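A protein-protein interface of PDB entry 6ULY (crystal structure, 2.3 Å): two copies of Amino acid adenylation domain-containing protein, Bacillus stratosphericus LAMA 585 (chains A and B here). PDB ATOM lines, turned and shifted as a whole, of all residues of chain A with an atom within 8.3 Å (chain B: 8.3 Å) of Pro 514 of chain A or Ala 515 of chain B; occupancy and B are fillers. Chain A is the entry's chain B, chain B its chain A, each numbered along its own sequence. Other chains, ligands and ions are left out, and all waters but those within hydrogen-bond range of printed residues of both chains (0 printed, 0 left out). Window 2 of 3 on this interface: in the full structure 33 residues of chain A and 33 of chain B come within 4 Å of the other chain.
The side-chain carboxylate (OE1) of Glu 513 of chain B sits at hydrogen-bond distance from the backbone NH (N) of Ala 515 of chain B, at 2.9 Å.
Among the printed residues, merely in contact across the chains: Gln 543 of chain A with Met 518 of chain B (3.4 Å), Pro 514 of chain A with Pro 514 of chain B (3.6 Å), Met 518 of chain A with Pro 514 of chain B (3.6 Å), Pro 514 of chain A with Met 518 of chain B (3.7 Å), Ala 515 of chain A with Pro 514 of chain B (3.8 Å), Pro 514 of chain A with Ala 515 of chain B (3.8 Å) and Met 518 of chain A with Tyr 512 of chain B (3.9 Å).
Ala 515 of chain B touches just one residue of chain A: Pro 514. Of the printed residues of chain A, Met 518 of chain B touches Pro 514 (3.7 Å) and Gln 543 (3.4 Å). Of the printed residues of chain B, Gln 543 of chain A touches Met 518 (3.4 Å). Printed residues of chain A within 4 Å of Tyr 512 of chain B: Met 518 (3.9 Å). Printed residues of chain B within 4 Å of Met 518 of chain A: Tyr 512 and Pro 514. The nearest printed residue of chain A that does not touch Tyr 512 of chain B is Ser 521 of chain A (7.0 Å).
Printed residues of chain A that touch a printed residue of chain B: Pro 514, Ala 515, Met 518 and Gln 543. Hydrophobic or aromatic side chains of chain B that line the printed part of chain A: Tyr 512, Pro 514 and Met 518. Among the printed residues, 7 pairs touch across the chains. Among the printed residues, no Asp or Glu carboxylate lies within 4 Å of a Lys or Arg side-chain nitrogen of the other chain.
Pro 514 of chain B touches its own counterpart, Pro 514 of chain A. Pro 514 of chain A touches Met 518 of chain B, and with the chains exchanged Met 518 of chain A touches Pro 514 of chain B. Met 518 of chain A touches Tyr 512 of chain B, but with the chains exchanged Tyr 512 of chain A does not touch Met 518 of chain B (6.7 Å). Gln 543 of chain A touches Met 518 of chain B, but with the chains exchanged Met 518 of chain A does not touch Gln 543 of chain B (4.6 Å). Positions printed for both chains: 511, 512, 513, 514, 515, 516, 517, 518, 519, 520, 521 and 543. Of the 7 pairs that touch across the chains among the printed residues, 5 have their exchanged pair printed and touching as well.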
ATOM      1  N   PRO A 509      16.131  -1.173   7.487  1.00  0.00           N
ATOM      2  CA  PRO A 509      17.383  -1.149   8.234  1.00  0.00           C
ATOM      3  C   PRO A 509      17.436   0.055   9.185  1.00  0.00           C
ATOM      4  O   PRO A 509      16.807   1.063   8.916  1.00  0.00           O
ATOM      5  CB  PRO A 509      18.454  -1.069   7.140  1.00  0.00           C
ATOM      6  CG  PRO A 509      17.763  -0.335   6.007  1.00  0.00           C
ATOM      7  CD  PRO A 509      16.305  -0.753   6.082  1.00  0.00           C
ATOM      8  N   LEU A 511      20.157   1.819   9.799  1.00  0.00           N
ATOM      9  CA  LEU A 511      20.943   2.821   9.041  1.00  0.00           C
ATOM     10  C   LEU A 511      20.993   2.398   7.576  1.00  0.00           C
ATOM     11  O   LEU A 511      21.240   1.212   7.294  1.00  0.00           O
ATOM     12  CB  LEU A 511      22.350   2.938   9.632  1.00  0.00           C
ATOM     13  CG  LEU A 511      23.052   4.271   9.379  1.00  0.00           C
ATOM     14  CD1 LEU A 511      22.610   5.315  10.400  1.00  0.00           C
ATOM     15  CD2 LEU A 511      24.565   4.099   9.396  1.00  0.00           C
ATOM     16  N   TYR A 512      20.780   3.358   6.679  1.00  0.00           N
ATOM     17  CA  TYR A 512      20.731   3.120   5.215  1.00  0.00           C
ATOM     18  C   TYR A 512      22.140   3.261   4.628  1.00  0.00           C
ATOM     19  O   TYR A 512      22.533   4.365   4.189  1.00  0.00           O
ATOM     20  CB  TYR A 512      19.708   4.053   4.572  1.00  0.00           C
ATOM     21  CG  TYR A 512      18.277   3.761   4.959  1.00  0.00           C
ATOM     22  CD1 TYR A 512      17.467   2.967   4.157  1.00  0.00           C
ATOM     23  CD2 TYR A 512      17.727   4.276   6.127  1.00  0.00           C
ATOM     24  CE1 TYR A 512      16.149   2.700   4.499  1.00  0.00           C
ATOM     25  CE2 TYR A 512      16.411   4.016   6.482  1.00  0.00           C
ATOM     26  CZ  TYR A 512      15.618   3.226   5.666  1.00  0.00           C
ATOM     27  OH  TYR A 512      14.321   2.973   6.013  1.00  0.00           O
ATOM     28  N   GLU A 513      22.883   2.151   4.637  1.00  0.00           N
ATOM     29  CA  GLU A 513      24.255   2.052   4.089  1.00  0.00           C
ATOM     30  C   GLU A 513      24.383   0.677   3.451  1.00  0.00           C
ATOM     31  O   GLU A 513      23.893  -0.291   4.020  1.00  0.00           O
ATOM     32  CB  GLU A 513      25.295   2.274   5.189  1.00  0.00           C
ATOM     33  CG  GLU A 513      26.671   2.673   4.674  1.00  0.00           C
ATOM     34  CD  GLU A 513      27.664   1.532   4.479  1.00  0.00           C
ATOM     35  OE1 GLU A 513      27.953   0.848   5.484  1.00  0.00           O
ATOM     36  OE2 GLU A 513      28.156   1.329   3.329  1.00  0.00           O
ATOM     37  N   PRO A 514      25.002   0.570   2.249  1.00  0.00           N
ATOM     38  CA  PRO A 514      25.061  -0.695   1.499  1.00  0.00           C
ATOM     39  C   PRO A 514      25.536  -1.959   2.247  1.00  0.00           C
ATOM     40  O   PRO A 514      24.840  -2.981   2.214  1.00  0.00           O
ATOM     41  CB  PRO A 514      26.069  -0.367   0.370  1.00  0.00           C
ATOM     42  CG  PRO A 514      25.940   1.127   0.147  1.00  0.00           C
ATOM     43  CD  PRO A 514      25.592   1.701   1.503  1.00  0.00           C
ATOM     44  N   ALA A 515      26.724  -1.894   2.857  1.00  0.00           N
ATOM     45  CA  ALA A 515      27.325  -3.004   3.630  1.00  0.00           C
ATOM     46  C   ALA A 515      26.499  -3.279   4.891  1.00  0.00           C
ATOM     47  O   ALA A 515      26.351  -4.452   5.240  1.00  0.00           O
ATOM     48  CB  ALA A 515      28.763  -2.690   3.969  1.00  0.00           C
ATOM     49  N   TYR A 516      25.966  -2.246   5.547  1.00  0.00           N
ATOM     50  CA  TYR A 516      25.132  -2.406   6.766  1.00  0.00           C
ATOM     51  C   TYR A 516      23.856  -3.183   6.411  1.00  0.00           C
ATOM     52  O   TYR A 516      23.482  -4.105   7.164  1.00  0.00           O
ATOM     53  CB  TYR A 516      24.798  -1.040   7.371  1.00  0.00           C
ATOM     54  CG  TYR A 516      24.063  -1.098   8.686  1.00  0.00           C
ATOM     55  CD1 TYR A 516      24.739  -0.988   9.890  1.00  0.00           C
ATOM     56  CD2 TYR A 516      22.688  -1.266   8.730  1.00  0.00           C
ATOM     57  CE1 TYR A 516      24.072  -1.041  11.102  1.00  0.00           C
ATOM     58  CE2 TYR A 516      22.005  -1.321   9.934  1.00  0.00           C
ATOM     59  CZ  TYR A 516      22.700  -1.208  11.125  1.00  0.00           C
ATOM     60  OH  TYR A 516      22.033  -1.262  12.315  1.00  0.00           O
ATOM     61  N   ILE A 517      23.214  -2.814   5.296  1.00  0.00           N
ATOM     62  CA  ILE A 517      21.955  -3.430   4.774  1.00  0.00           C
ATOM     63  C   ILE A 517      22.196  -4.870   4.299  1.00  0.00           C
ATOM     64  O   ILE A 517      21.351  -5.738   4.597  1.00  0.00           O
ATOM     65  CB  ILE A 517      21.367  -2.564   3.641  1.00  0.00           C
ATOM     66  CG1 ILE A 517      20.725  -1.282   4.179  1.00  0.00           C
ATOM     67  CG2 ILE A 517      20.394  -3.370   2.795  1.00  0.00           C
ATOM     68  CD1 ILE A 517      20.603  -0.181   3.152  1.00  0.00           C
ATOM     69  N   MET A 518      23.304  -5.104   3.588  1.00  0.00           N
ATOM     70  CA  MET A 518      23.682  -6.411   2.979  1.00  0.00           C
ATOM     71  C   MET A 518      23.920  -7.480   4.053  1.00  0.00           C
ATOM     72  O   MET A 518      23.526  -8.642   3.828  1.00  0.00           O
ATOM     73  CB  MET A 518      24.950  -6.265   2.131  1.00  0.00           C
ATOM     74  CG  MET A 518      25.066  -7.310   1.036  1.00  0.00           C
ATOM     75  SD  MET A 518      26.778  -7.580   0.509  1.00  0.00           S
ATOM     76  CE  MET A 518      27.480  -8.268   2.007  1.00  0.00           C
ATOM     77  N   ARG A 519      24.541  -7.095   5.170  1.00  0.00           N
ATOM     78  CA  ARG A 519      24.914  -8.003   6.292  1.00  0.00           C
ATOM     79  C   ARG A 519      23.706  -8.225   7.223  1.00  0.00           C
ATOM     80  O   ARG A 519      23.518  -9.374   7.649  1.00  0.00           O
ATOM     81  CB  ARG A 519      26.180  -7.498   7.005  1.00  0.00           C
ATOM     82  CG  ARG A 519      26.865  -8.558   7.861  1.00  0.00           C
ATOM     83  CD  ARG A 519      28.390  -8.608   7.802  1.00  0.00           C
ATOM     84  NE  ARG A 519      28.870  -9.893   8.316  1.00  0.00           N
ATOM     85  CZ  ARG A 519      28.990 -10.221   9.607  1.00  0.00           C
ATOM     86  NH1 ARG A 519      28.689  -9.352  10.560  1.00  0.00           N
ATOM     87  NH2 ARG A 519      29.406 -11.431   9.945  1.00  0.00           N
ATOM     88  N   ALA A 520      22.895  -7.205   7.531  1.00  0.00           N
ATOM     89  CA  ALA A 520      21.587  -7.409   8.203  1.00  0.00           C
ATOM     90  C   ALA A 520      20.747  -8.379   7.362  1.00  0.00           C
ATOM     91  O   ALA A 520      20.093  -9.262   7.936  1.00  0.00           O
ATOM     92  CB  ALA A 520      20.862  -6.102   8.417  1.00  0.00           C
ATOM     93  N   SER A 521      20.786  -8.230   6.038  1.00  0.00           N
ATOM     94  CA  SER A 521      20.111  -9.141   5.080  1.00  0.00           C
ATOM     95  C   SER A 521      20.686 -10.559   5.195  1.00  0.00           C
ATOM     96  O   SER A 521      19.915 -11.520   5.050  1.00  0.00           O
ATOM     97  CB  SER A 521      20.217  -8.615   3.671  1.00  0.00           C
ATOM     98  OG  SER A 521      19.607  -9.505   2.748  1.00  0.00           O
ATOM     99  N   GLN A 543      15.003  -4.916   1.447  1.00  0.00           N
ATOM    100  CA  GLN A 543      15.037  -3.694   2.294  1.00  0.00           C
ATOM    101  C   GLN A 543      14.153  -2.614   1.658  1.00  0.00           C
ATOM    102  O   GLN A 543      14.052  -2.623   0.415  1.00  0.00           O
ATOM    103  CB  GLN A 543      16.475  -3.199   2.456  1.00  0.00           C
ATOM    104  CG  GLN A 543      17.042  -2.551   1.201  1.00  0.00           C
ATOM    105  CD  GLN A 543      17.026  -1.044   1.279  1.00  0.00           C
ATOM    106  OE1 GLN A 543      16.180  -0.446   1.941  1.00  0.00           O
ATOM    107  NE2 GLN A 543      17.970  -0.415   0.598  1.00  0.00           N
ATOM    108  N   LEU B 511      29.680  -8.301 -10.117  1.00  0.00           N
ATOM    109  CA  LEU B 511      30.508  -8.042  -8.924  1.00  0.00           C
ATOM    110  C   LEU B 511      29.622  -8.177  -7.698  1.00  0.00           C
ATOM    111  O   LEU B 511      28.641  -7.434  -7.610  1.00  0.00           O
ATOM    112  CB  LEU B 511      31.072  -6.628  -9.017  1.00  0.00           C
ATOM    113  CG  LEU B 511      32.292  -6.375  -8.153  1.00  0.00           C
ATOM    114  CD1 LEU B 511      33.471  -7.177  -8.685  1.00  0.00           C
ATOM    115  CD2 LEU B 511      32.589  -4.892  -8.122  1.00  0.00           C
ATOM    116  N   TYR B 512      29.949  -9.100  -6.798  1.00  0.00           N
ATOM    117  CA  TYR B 512      29.204  -9.257  -5.528  1.00  0.00           C
ATOM    118  C   TYR B 512      29.820  -8.305  -4.491  1.00  0.00           C
ATOM    119  O   TYR B 512      30.483  -8.749  -3.534  1.00  0.00           O
ATOM    120  CB  TYR B 512      29.125 -10.729  -5.109  1.00  0.00           C
ATOM    121  CG  TYR B 512      28.027 -10.989  -4.105  1.00  0.00           C
ATOM    122  CD1 TYR B 512      28.059 -10.380  -2.855  1.00  0.00           C
ATOM    123  CD2 TYR B 512      26.927 -11.783  -4.407  1.00  0.00           C
ATOM    124  CE1 TYR B 512      27.053 -10.574  -1.924  1.00  0.00           C
ATOM    125  CE2 TYR B 512      25.909 -11.988  -3.484  1.00  0.00           C
ATOM    126  CZ  TYR B 512      25.973 -11.383  -2.236  1.00  0.00           C
ATOM    127  OH  TYR B 512      24.982 -11.577  -1.313  1.00  0.00           O
ATOM    128  N   GLU B 513      29.604  -7.006  -4.708  1.00  0.00           N
ATOM    129  CA  GLU B 513      29.911  -5.901  -3.773  1.00  0.00           C
ATOM    130  C   GLU B 513      28.592  -5.216  -3.432  1.00  0.00           C
ATOM    131  O   GLU B 513      27.765  -5.016  -4.321  1.00  0.00           O
ATOM    132  CB  GLU B 513      30.917  -4.968  -4.445  1.00  0.00           C
ATOM    133  CG  GLU B 513      31.646  -4.049  -3.478  1.00  0.00           C
ATOM    134  CD  GLU B 513      30.952  -2.713  -3.257  1.00  0.00           C
ATOM    135  OE1 GLU B 513      29.938  -2.480  -3.943  1.00  0.00           O
ATOM    136  OE2 GLU B 513      31.427  -1.902  -2.413  1.00  0.00           O
ATOM    137  N   PRO B 514      28.328  -4.864  -2.151  1.00  0.00           N
ATOM    138  CA  PRO B 514      26.995  -4.407  -1.750  1.00  0.00           C
ATOM    139  C   PRO B 514      26.440  -3.210  -2.550  1.00  0.00           C
ATOM    140  O   PRO B 514      25.270  -3.245  -2.943  1.00  0.00           O
ATOM    141  CB  PRO B 514      27.157  -4.056  -0.255  1.00  0.00           C
ATOM    142  CG  PRO B 514      28.651  -3.980   0.002  1.00  0.00           C
ATOM    143  CD  PRO B 514      29.269  -4.909  -1.020  1.00  0.00           C
ATOM    144  N   ALA B 515      27.247  -2.169  -2.784  1.00  0.00           N
ATOM    145  CA  ALA B 515      26.794  -0.997  -3.572  1.00  0.00           C
ATOM    146  C   ALA B 515      26.472  -1.436  -5.007  1.00  0.00           C
ATOM    147  O   ALA B 515      25.417  -1.030  -5.556  1.00  0.00           O
ATOM    148  CB  ALA B 515      27.821   0.111  -3.547  1.00  0.00           C
ATOM    149  N   TYR B 516      27.351  -2.241  -5.599  1.00  0.00           N
ATOM    150  CA  TYR B 516      27.193  -2.727  -6.987  1.00  0.00           C
ATOM    151  C   TYR B 516      25.874  -3.489  -7.097  1.00  0.00           C
ATOM    152  O   TYR B 516      25.170  -3.336  -8.110  1.00  0.00           O
ATOM    153  CB  TYR B 516      28.365  -3.622  -7.406  1.00  0.00           C
ATOM    154  CG  TYR B 516      28.464  -3.840  -8.899  1.00  0.00           C
ATOM    155  CD1 TYR B 516      29.101  -2.913  -9.717  1.00  0.00           C
ATOM    156  CD2 TYR B 516      27.890  -4.947  -9.514  1.00  0.00           C
ATOM    157  CE1 TYR B 516      29.174  -3.078 -11.095  1.00  0.00           C
ATOM    158  CE2 TYR B 516      27.970  -5.140 -10.888  1.00  0.00           C
ATOM    159  CZ  TYR B 516      28.604  -4.197 -11.685  1.00  0.00           C
ATOM    160  OH  TYR B 516      28.672  -4.372 -13.041  1.00  0.00           O
ATOM    161  N   ILE B 517      25.560  -4.300  -6.094  1.00  0.00           N
ATOM    162  CA  ILE B 517      24.331  -5.141  -6.108  1.00  0.00           C
ATOM    163  C   ILE B 517      23.102  -4.233  -5.991  1.00  0.00           C
ATOM    164  O   ILE B 517      22.113  -4.462  -6.721  1.00  0.00           O
ATOM    165  CB  ILE B 517      24.371  -6.211  -5.001  1.00  0.00           C
ATOM    166  CG1 ILE B 517      25.430  -7.278  -5.301  1.00  0.00           C
ATOM    167  CG2 ILE B 517      22.991  -6.839  -4.806  1.00  0.00           C
ATOM    168  CD1 ILE B 517      25.776  -8.165  -4.116  1.00  0.00           C
ATOM    169  N   MET B 518      23.148  -3.243  -5.104  1.00  0.00           N
ATOM    170  CA  MET B 518      22.000  -2.332  -4.901  1.00  0.00           C
ATOM    171  C   MET B 518      21.779  -1.490  -6.163  1.00  0.00           C
ATOM    172  O   MET B 518      20.610  -1.270  -6.520  1.00  0.00           O
ATOM    173  CB  MET B 518      22.220  -1.459  -3.666  1.00  0.00           C
ATOM    174  CG  MET B 518      21.977  -2.236  -2.384  1.00  0.00           C
ATOM    175  SD  MET B 518      22.246  -1.273  -0.891  1.00  0.00           S
ATOM    176  CE  MET B 518      20.925  -0.068  -1.048  1.00  0.00           C
ATOM    177  N   ARG B 519      22.841  -1.090  -6.857  1.00  0.00           N
ATOM    178  CA  ARG B 519      22.689  -0.350  -8.132  1.00  0.00           C
ATOM    179  C   ARG B 519      21.986  -1.235  -9.173  1.00  0.00           C
ATOM    180  O   ARG B 519      20.980  -0.781  -9.773  1.00  0.00           O
ATOM    181  CB  ARG B 519      24.042   0.100  -8.669  1.00  0.00           C
ATOM    182  CG  ARG B 519      23.939   0.809 -10.008  1.00  0.00           C
ATOM    183  CD  ARG B 519      25.293   0.919 -10.672  1.00  0.00           C
ATOM    184  NE  ARG B 519      26.298   1.346  -9.711  1.00  0.00           N
ATOM    185  CZ  ARG B 519      27.594   1.131  -9.828  1.00  0.00           C
ATOM    186  NH1 ARG B 519      28.055   0.488 -10.887  1.00  0.00           N
ATOM    187  NH2 ARG B 519      28.415   1.565  -8.883  1.00  0.00           N
ATOM    188  N   ALA B 520      22.485  -2.451  -9.398  1.00  0.00           N
ATOM    189  CA  ALA B 520      21.905  -3.360 -10.410  1.00  0.00           C
ATOM    190  C   ALA B 520      20.439  -3.629 -10.068  1.00  0.00           C
ATOM    191  O   ALA B 520      19.621  -3.616 -11.002  1.00  0.00           O
ATOM    192  CB  ALA B 520      22.689  -4.642 -10.518  1.00  0.00           C
ATOM    193  N   SER B 521      20.122  -3.858  -8.787  1.00  0.00           N
ATOM    194  CA  SER B 521      18.748  -4.192  -8.318  1.00  0.00           C
ATOM    195  C   SER B 521      17.778  -3.057  -8.652  1.00  0.00           C
ATOM    196  O   SER B 521      16.669  -3.340  -9.144  1.00  0.00           O
ATOM    197  CB  SER B 521      18.736  -4.496  -6.846  1.00  0.00           C
ATOM    198  OG  SER B 521      19.516  -5.651  -6.584  1.00  0.00           O
ATOM    199  N   GLN B 522      18.190  -1.813  -8.401  1.00  0.00           N
ATOM    200  CA  GLN B 522      17.387  -0.610  -8.731  1.00  0.00           C
ATOM    201  C   GLN B 522      17.184  -0.548 -10.247  1.00  0.00           C
ATOM    202  O   GLN B 522      16.046  -0.314 -10.665  1.00  0.00           O
ATOM    203  CB  GLN B 522      18.055   0.687  -8.265  1.00  0.00           C
ATOM    204  CG  GLN B 522      18.159   0.857  -6.755  1.00  0.00           C
ATOM    205  CD  GLN B 522      18.969   2.087  -6.406  1.00  0.00           C
ATOM    206  OE1 GLN B 522      19.894   2.041  -5.600  1.00  0.00           O
ATOM    207  NE2 GLN B 522      18.642   3.208  -7.030  1.00  0.00           N
ATOM    208  N   GLN B 543      19.802 -11.081  -5.461  1.00  0.00           N
ATOM    209  CA  GLN B 543      21.201 -11.419  -5.812  1.00  0.00           C
ATOM    210  C   GLN B 543      21.477 -12.886  -5.457  1.00  0.00           C
ATOM    211  O   GLN B 543      20.950 -13.372  -4.434  1.00  0.00           O
ATOM    212  CB  GLN B 543      22.171 -10.459  -5.122  1.00  0.00           C
ATOM    213  CG  GLN B 543      22.256 -10.606  -3.602  1.00  0.00           C
ATOM    214  CD  GLN B 543      21.432  -9.589  -2.842  1.00  0.00           C
ATOM    215  OE1 GLN B 543      20.396  -9.118  -3.312  1.00  0.00           O
ATOM    216  NE2 GLN B 543      21.909  -9.214  -1.660  1.00  0.00           N
